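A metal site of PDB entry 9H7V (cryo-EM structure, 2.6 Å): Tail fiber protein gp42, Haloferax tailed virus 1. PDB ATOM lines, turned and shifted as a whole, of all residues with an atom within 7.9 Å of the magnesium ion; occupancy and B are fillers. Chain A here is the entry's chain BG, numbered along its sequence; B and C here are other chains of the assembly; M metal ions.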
ATOM      1  N   ALA A   9     -19.248   4.840  -7.363  1.00  0.00           N
ATOM      2  CA  ALA A   9     -19.744   5.972  -8.140  1.00  0.00           C
ATOM      3  C   ALA A   9     -19.700   5.651  -9.638  1.00  0.00           C
ATOM      4  O   ALA A   9     -18.805   4.950 -10.086  1.00  0.00           O
ATOM      5  CB  ALA A   9     -18.909   7.187  -7.826  1.00  0.00           C
ATOM      6  N   VAL A  10     -20.684   6.182 -10.389  1.00  0.00           N
ATOM      7  CA  VAL A  10     -20.743   5.985 -11.830  1.00  0.00           C
ATOM      8  C   VAL A  10     -20.896   7.328 -12.554  1.00  0.00           C
ATOM      9  O   VAL A  10     -21.620   8.214 -12.093  1.00  0.00           O
ATOM     10  CB  VAL A  10     -21.814   4.964 -12.262  1.00  0.00           C
ATOM     11  CG1 VAL A  10     -21.446   3.534 -11.873  1.00  0.00           C
ATOM     12  CG2 VAL A  10     -23.215   5.301 -11.772  1.00  0.00           C
ATOM     13  N   VAL A  11     -20.206   7.439 -13.702  1.00  0.00           N
ATOM     14  CA  VAL A  11     -20.148   8.624 -14.543  1.00  0.00           C
ATOM     15  C   VAL A  11     -20.669   8.250 -15.928  1.00  0.00           C
ATOM     16  O   VAL A  11     -20.281   7.227 -16.484  1.00  0.00           O
ATOM     17  CB  VAL A  11     -18.706   9.176 -14.637  1.00  0.00           C
ATOM     18  CG1 VAL A  11     -18.606  10.398 -15.546  1.00  0.00           C
ATOM     19  CG2 VAL A  11     -18.123   9.498 -13.278  1.00  0.00           C
ATOM     20  N   PHE A  12     -21.559   9.099 -16.480  1.00  0.00           N
ATOM     21  CA  PHE A  12     -22.167   8.900 -17.781  1.00  0.00           C
ATOM     22  C   PHE A  12     -22.494  10.259 -18.391  1.00  0.00           C
ATOM     23  O   PHE A  12     -22.829  11.171 -17.647  1.00  0.00           O
ATOM     24  CB  PHE A  12     -23.443   8.068 -17.631  1.00  0.00           C
ATOM     25  CG  PHE A  12     -24.161   7.752 -18.917  1.00  0.00           C
ATOM     26  CD1 PHE A  12     -23.762   6.664 -19.689  1.00  0.00           C
ATOM     27  CD2 PHE A  12     -25.212   8.536 -19.363  1.00  0.00           C
ATOM     28  CE1 PHE A  12     -24.408   6.374 -20.881  1.00  0.00           C
ATOM     29  CE2 PHE A  12     -25.862   8.239 -20.551  1.00  0.00           C
ATOM     30  CZ  PHE A  12     -25.462   7.156 -21.314  1.00  0.00           C
ATOM     31  N   PRO A  13     -22.451  10.477 -19.735  1.00  0.00           N
ATOM     32  CA  PRO A  13     -21.895   9.532 -20.714  1.00  0.00           C
ATOM     33  C   PRO A  13     -20.415   9.756 -21.052  1.00  0.00           C
ATOM     34  O   PRO A  13     -19.918  10.873 -20.891  1.00  0.00           O
ATOM     35  CB  PRO A  13     -22.797   9.816 -21.921  1.00  0.00           C
ATOM     36  CG  PRO A  13     -23.075  11.307 -21.852  1.00  0.00           C
ATOM     37  CD  PRO A  13     -23.032  11.663 -20.388  1.00  0.00           C
ATOM     38  N   GLN A  14     -19.720   8.711 -21.535  1.00  0.00           N
ATOM     39  CA  GLN A  14     -18.288   8.765 -21.789  1.00  0.00           C
ATOM     40  C   GLN A  14     -17.913   8.028 -23.087  1.00  0.00           C
ATOM     41  O   GLN A  14     -18.340   6.893 -23.295  1.00  0.00           O
ATOM     42  CB  GLN A  14     -17.489   8.230 -20.580  1.00  0.00           C
ATOM     43  CG  GLN A  14     -17.669   9.032 -19.304  1.00  0.00           C
ATOM     44  CD  GLN A  14     -16.942   8.448 -18.106  1.00  0.00           C
ATOM     45  OE1 GLN A  14     -17.339   7.434 -17.552  1.00  0.00           O
ATOM     46  NE2 GLN A  14     -15.872   9.114 -17.704  1.00  0.00           N
ATOM     47  N   ASP A  15     -17.102   8.694 -23.927  1.00  0.00           N
ATOM     48  CA  ASP A  15     -16.657   8.274 -25.254  1.00  0.00           C
ATOM     49  C   ASP A  15     -15.156   8.516 -25.419  1.00  0.00           C
ATOM     50  O   ASP A  15     -14.555   9.201 -24.594  1.00  0.00           O
ATOM     51  CB  ASP A  15     -17.165   9.236 -26.336  1.00  0.00           C
ATOM     52  CG  ASP A  15     -18.642   9.265 -26.643  1.00  0.00           C
ATOM     53  OD1 ASP A  15     -19.384   8.369 -26.170  1.00  0.00           O
ATOM     54  OD2 ASP A  15     -19.052  10.180 -27.375  1.00  0.00           O
ATOM     55  N   VAL A  20     -11.655   9.449 -22.340  1.00  0.00           N
ATOM     56  CA  VAL A  20     -11.411   8.020 -22.103  1.00  0.00           C
ATOM     57  C   VAL A  20     -10.801   7.380 -23.347  1.00  0.00           C
ATOM     58  O   VAL A  20     -10.958   7.901 -24.457  1.00  0.00           O
ATOM     59  CB  VAL A  20     -12.651   7.235 -21.612  1.00  0.00           C
ATOM     60  CG1 VAL A  20     -13.088   7.567 -20.193  1.00  0.00           C
ATOM     61  CG2 VAL A  20     -13.835   7.234 -22.568  1.00  0.00           C
ATOM     62  N   ASP A  24     -12.882   1.867 -23.451  1.00  0.00           N
ATOM     63  CA  ASP A  24     -13.374   2.285 -22.144  1.00  0.00           C
ATOM     64  C   ASP A  24     -14.709   3.034 -22.216  1.00  0.00           C
ATOM     65  O   ASP A  24     -15.164   3.539 -21.192  1.00  0.00           O
ATOM     66  CB  ASP A  24     -12.327   3.141 -21.415  1.00  0.00           C
ATOM     67  CG  ASP A  24     -10.968   2.479 -21.221  1.00  0.00           C
ATOM     68  OD1 ASP A  24     -10.921   1.232 -21.143  1.00  0.00           O
ATOM     69  OD2 ASP A  24      -9.976   3.230 -21.137  1.00  0.00           O
ATOM     70  N   GLU A  25     -15.335   3.113 -23.404  1.00  0.00           N
ATOM     71  CA  GLU A  25     -16.563   3.867 -23.593  1.00  0.00           C
ATOM     72  C   GLU A  25     -17.698   3.234 -22.769  1.00  0.00           C
ATOM     73  O   GLU A  25     -17.751   2.012 -22.640  1.00  0.00           O
ATOM     74  CB  GLU A  25     -16.897   3.980 -25.075  1.00  0.00           C
ATOM     75  CG  GLU A  25     -15.797   4.633 -25.899  1.00  0.00           C
ATOM     76  CD  GLU A  25     -16.077   4.887 -27.367  1.00  0.00           C
ATOM     77  OE1 GLU A  25     -16.407   6.032 -27.730  1.00  0.00           O
ATOM     78  OE2 GLU A  25     -15.921   3.939 -28.167  1.00  0.00           O
ATOM     79  N   ASP A  26     -18.582   4.080 -22.204  1.00  0.00           N
ATOM     80  CA  ASP A  26     -19.682   3.656 -21.341  1.00  0.00           C
ATOM     81  C   ASP A  26     -20.634   2.725 -22.103  1.00  0.00           C
ATOM     82  O   ASP A  26     -20.764   2.837 -23.315  1.00  0.00           O
ATOM     83  CB  ASP A  26     -20.499   4.852 -20.856  1.00  0.00           C
ATOM     84  CG  ASP A  26     -19.983   5.551 -19.602  1.00  0.00           C
ATOM     85  OD1 ASP A  26     -19.371   4.882 -18.746  1.00  0.00           O
ATOM     86  OD2 ASP A  26     -20.227   6.772 -19.490  1.00  0.00           O
ATOM     87  N   TYR A  27     -21.305   1.835 -21.359  1.00  0.00           N
ATOM     88  CA  TYR A  27     -22.374   1.025 -21.907  1.00  0.00           C
ATOM     89  C   TYR A  27     -23.690   1.807 -21.861  1.00  0.00           C
ATOM     90  O   TYR A  27     -23.869   2.713 -21.043  1.00  0.00           O
ATOM     91  CB  TYR A  27     -22.455  -0.350 -21.238  1.00  0.00           C
ATOM     92  CG  TYR A  27     -21.801  -1.470 -22.009  1.00  0.00           C
ATOM     93  CD1 TYR A  27     -20.431  -1.694 -21.928  1.00  0.00           C
ATOM     94  CD2 TYR A  27     -22.546  -2.314 -22.811  1.00  0.00           C
ATOM     95  CE1 TYR A  27     -19.829  -2.722 -22.628  1.00  0.00           C
ATOM     96  CE2 TYR A  27     -21.962  -3.354 -23.523  1.00  0.00           C
ATOM     97  CZ  TYR A  27     -20.591  -3.557 -23.430  1.00  0.00           C
ATOM     98  OH  TYR A  27     -19.992  -4.568 -24.127  1.00  0.00           O
ATOM     99  N   TYR A  32     -29.197   5.032 -17.445  1.00  0.00           N
ATOM    100  CA  TYR A  32     -28.237   6.097 -17.699  1.00  0.00           C
ATOM    101  C   TYR A  32     -28.867   7.173 -18.583  1.00  0.00           C
ATOM    102  O   TYR A  32     -28.659   8.366 -18.331  1.00  0.00           O
ATOM    103  CB  TYR A  32     -26.982   5.555 -18.364  1.00  0.00           C
ATOM    104  CG  TYR A  32     -25.902   4.970 -17.482  1.00  0.00           C
ATOM    105  CD1 TYR A  32     -25.619   5.472 -16.215  1.00  0.00           C
ATOM    106  CD2 TYR A  32     -25.126   3.927 -17.955  1.00  0.00           C
ATOM    107  CE1 TYR A  32     -24.612   4.921 -15.435  1.00  0.00           C
ATOM    108  CE2 TYR A  32     -24.108   3.374 -17.189  1.00  0.00           C
ATOM    109  CZ  TYR A  32     -23.854   3.866 -15.920  1.00  0.00           C
ATOM    110  OH  TYR A  32     -22.856   3.318 -15.163  1.00  0.00           O
ATOM    111  N   TYR A 102     -22.133  15.651 -17.628  1.00  0.00           N
ATOM    112  CA  TYR A 102     -22.093  14.289 -17.132  1.00  0.00           C
ATOM    113  C   TYR A 102     -23.133  14.163 -16.012  1.00  0.00           C
ATOM    114  O   TYR A 102     -23.489  15.160 -15.392  1.00  0.00           O
ATOM    115  CB  TYR A 102     -20.747  13.981 -16.468  1.00  0.00           C
ATOM    116  CG  TYR A 102     -19.501  13.963 -17.310  1.00  0.00           C
ATOM    117  CD1 TYR A 102     -19.299  13.015 -18.301  1.00  0.00           C
ATOM    118  CD2 TYR A 102     -18.461  14.845 -17.041  1.00  0.00           C
ATOM    119  CE1 TYR A 102     -18.119  12.982 -19.044  1.00  0.00           C
ATOM    120  CE2 TYR A 102     -17.273  14.825 -17.759  1.00  0.00           C
ATOM    121  CZ  TYR A 102     -17.111  13.888 -18.767  1.00  0.00           C
ATOM    122  OH  TYR A 102     -15.956  13.849 -19.500  1.00  0.00           O
ATOM    123  N   VAL A 103     -23.603  12.930 -15.765  1.00  0.00           N
ATOM    124  CA  VAL A 103     -24.278  12.597 -14.523  1.00  0.00           C
ATOM    125  C   VAL A 103     -23.307  11.813 -13.665  1.00  0.00           C
ATOM    126  O   VAL A 103     -22.694  10.849 -14.132  1.00  0.00           O
ATOM    127  CB  VAL A 103     -25.585  11.791 -14.720  1.00  0.00           C
ATOM    128  CG1 VAL A 103     -26.460  11.822 -13.477  1.00  0.00           C
ATOM    129  CG2 VAL A 103     -26.379  12.272 -15.924  1.00  0.00           C
ATOM    130  N   VAL A 127     -14.564  14.553 -11.160  1.00  0.00           N
ATOM    131  CA  VAL A 127     -14.458  13.430 -12.074  1.00  0.00           C
ATOM    132  C   VAL A 127     -13.066  13.473 -12.699  1.00  0.00           C
ATOM    133  O   VAL A 127     -12.543  14.553 -12.949  1.00  0.00           O
ATOM    134  CB  VAL A 127     -15.563  13.511 -13.156  1.00  0.00           C
ATOM    135  CG1 VAL A 127     -15.440  12.419 -14.222  1.00  0.00           C
ATOM    136  CG2 VAL A 127     -16.960  13.481 -12.537  1.00  0.00           C
ATOM    137  N   SER A 131     -10.312   7.944 -17.324  1.00  0.00           N
ATOM    138  CA  SER A 131     -10.742   6.576 -17.086  1.00  0.00           C
ATOM    139  C   SER A 131     -12.217   6.569 -16.703  1.00  0.00           C
ATOM    140  O   SER A 131     -12.741   7.572 -16.224  1.00  0.00           O
ATOM    141  CB  SER A 131      -9.881   5.924 -16.031  1.00  0.00           C
ATOM    142  OG  SER A 131     -10.210   4.553 -15.891  1.00  0.00           O
ATOM    143  N   ASN A 132     -12.882   5.415 -16.912  1.00  0.00           N
ATOM    144  CA  ASN A 132     -14.320   5.308 -16.756  1.00  0.00           C
ATOM    145  C   ASN A 132     -14.697   5.230 -15.283  1.00  0.00           C
ATOM    146  O   ASN A 132     -14.141   4.415 -14.544  1.00  0.00           O
ATOM    147  CB  ASN A 132     -14.889   4.140 -17.575  1.00  0.00           C
ATOM    148  CG  ASN A 132     -16.369   4.268 -17.877  1.00  0.00           C
ATOM    149  OD1 ASN A 132     -17.166   4.606 -17.012  1.00  0.00           O
ATOM    150  ND2 ASN A 132     -16.743   3.974 -19.112  1.00  0.00           N
ATOM    151  N   ASP A 133     -15.616   6.115 -14.859  1.00  0.00           N
ATOM    152  CA  ASP A 133     -16.316   6.091 -13.578  1.00  0.00           C
ATOM    153  C   ASP A 133     -15.412   6.394 -12.375  1.00  0.00           C
ATOM    154  O   ASP A 133     -15.802   6.123 -11.240  1.00  0.00           O
ATOM    155  CB  ASP A 133     -17.153   4.812 -13.397  1.00  0.00           C
ATOM    156  CG  ASP A 133     -18.372   4.705 -14.283  1.00  0.00           C
ATOM    157  OD1 ASP A 133     -18.656   5.662 -15.028  1.00  0.00           O
ATOM    158  OD2 ASP A 133     -19.050   3.653 -14.226  1.00  0.00           O
ATOM    159  N   SER A 134     -14.236   6.980 -12.608  1.00  0.00           N
ATOM    160  CA  SER A 134     -13.372   7.397 -11.503  1.00  0.00           C
ATOM    161  C   SER A 134     -13.812   8.760 -10.963  1.00  0.00           C
ATOM    162  O   SER A 134     -13.706   9.765 -11.661  1.00  0.00           O
ATOM    163  CB  SER A 134     -11.909   7.360 -11.881  1.00  0.00           C
ATOM    164  OG  SER A 134     -11.703   7.899 -13.179  1.00  0.00           O
ATOM    165  N   GLN B  85     -25.119  -0.404 -15.780  1.00  0.00           N
ATOM    166  CA  GLN B  85     -23.855  -1.074 -16.012  1.00  0.00           C
ATOM    167  C   GLN B  85     -22.704  -0.156 -15.607  1.00  0.00           C
ATOM    168  O   GLN B  85     -22.565   0.928 -16.169  1.00  0.00           O
ATOM    169  CB  GLN B  85     -23.744  -1.460 -17.494  1.00  0.00           C
ATOM    170  CG  GLN B  85     -24.776  -2.495 -17.953  1.00  0.00           C
ATOM    171  CD  GLN B  85     -25.170  -2.366 -19.402  1.00  0.00           C
ATOM    172  OE1 GLN B  85     -25.698  -1.356 -19.844  1.00  0.00           O
ATOM    173  NE2 GLN B  85     -24.937  -3.424 -20.165  1.00  0.00           N
ATOM    174  N   SER B  86     -21.889  -0.602 -14.639  1.00  0.00           N
ATOM    175  CA  SER B  86     -20.712   0.136 -14.202  1.00  0.00           C
ATOM    176  C   SER B  86     -19.622   0.082 -15.273  1.00  0.00           C
ATOM    177  O   SER B  86     -19.438  -0.960 -15.900  1.00  0.00           O
ATOM    178  CB  SER B  86     -20.196  -0.396 -12.887  1.00  0.00           C
ATOM    179  OG  SER B  86     -18.998   0.254 -12.502  1.00  0.00           O
ATOM    180  N   GLY B  87     -18.933   1.215 -15.472  1.00  0.00           N
ATOM    181  CA  GLY B  87     -17.753   1.305 -16.307  1.00  0.00           C
ATOM    182  C   GLY B  87     -17.976   0.831 -17.736  1.00  0.00           C
ATOM    183  O   GLY B  87     -18.948   1.218 -18.378  1.00  0.00           O
ATOM    184  N   SER B  88     -17.062  -0.022 -18.213  1.00  0.00           N
ATOM    185  CA  SER B  88     -17.120  -0.612 -19.545  1.00  0.00           C
ATOM    186  C   SER B  88     -17.593  -2.061 -19.473  1.00  0.00           C
ATOM    187  O   SER B  88     -17.307  -2.855 -20.372  1.00  0.00           O
ATOM    188  CB  SER B  88     -15.780  -0.479 -20.251  1.00  0.00           C
ATOM    189  OG  SER B  88     -14.753  -1.099 -19.498  1.00  0.00           O
ATOM    190  N   LEU C   4     -21.106   3.242 -26.191  1.00  0.00           N
ATOM    191  CA  LEU C   4     -21.312   4.488 -26.904  1.00  0.00           C
ATOM    192  C   LEU C   4     -20.264   4.607 -28.010  1.00  0.00           C
ATOM    193  O   LEU C   4     -19.132   4.155 -27.828  1.00  0.00           O
ATOM    194  CB  LEU C   4     -21.200   5.676 -25.938  1.00  0.00           C
ATOM    195  CG  LEU C   4     -22.150   5.693 -24.735  1.00  0.00           C
ATOM    196  CD1 LEU C   4     -21.982   6.984 -23.959  1.00  0.00           C
ATOM    197  CD2 LEU C   4     -23.600   5.501 -25.142  1.00  0.00           C
HETATM  198 MG    MG M   1     -18.730   5.956 -17.039  1.00  0.00          MG
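The magnesium ion is bound by OD1 of Asp 133, OD1 of Asn 132, O of Val 11, OE1 of Gln 14 and OD1 of Asp 26.
Five residues have an atom within 4 Å of the magnesium ion: Val 11, Gln 14, Asp 26, Asn 132 and Asp 133. The nearest printed residue that does not touch the magnesium ion is Phe 12 (4.3 Å).
The side-chain carboxylate of Asp 133 is in hydrogen-bond range of the backbone NH of Gly 87 of chain B, at 2.7 Å. The side-chain amide nitrogen of Asn 132 sits at hydrogen-bond distance from the backbone carbonyl oxygen of Asp 24 (2.6 Å). N of Leu 4 of chain C sits at hydrogen-bond distance from O of Asp 26 (2.9 Å).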
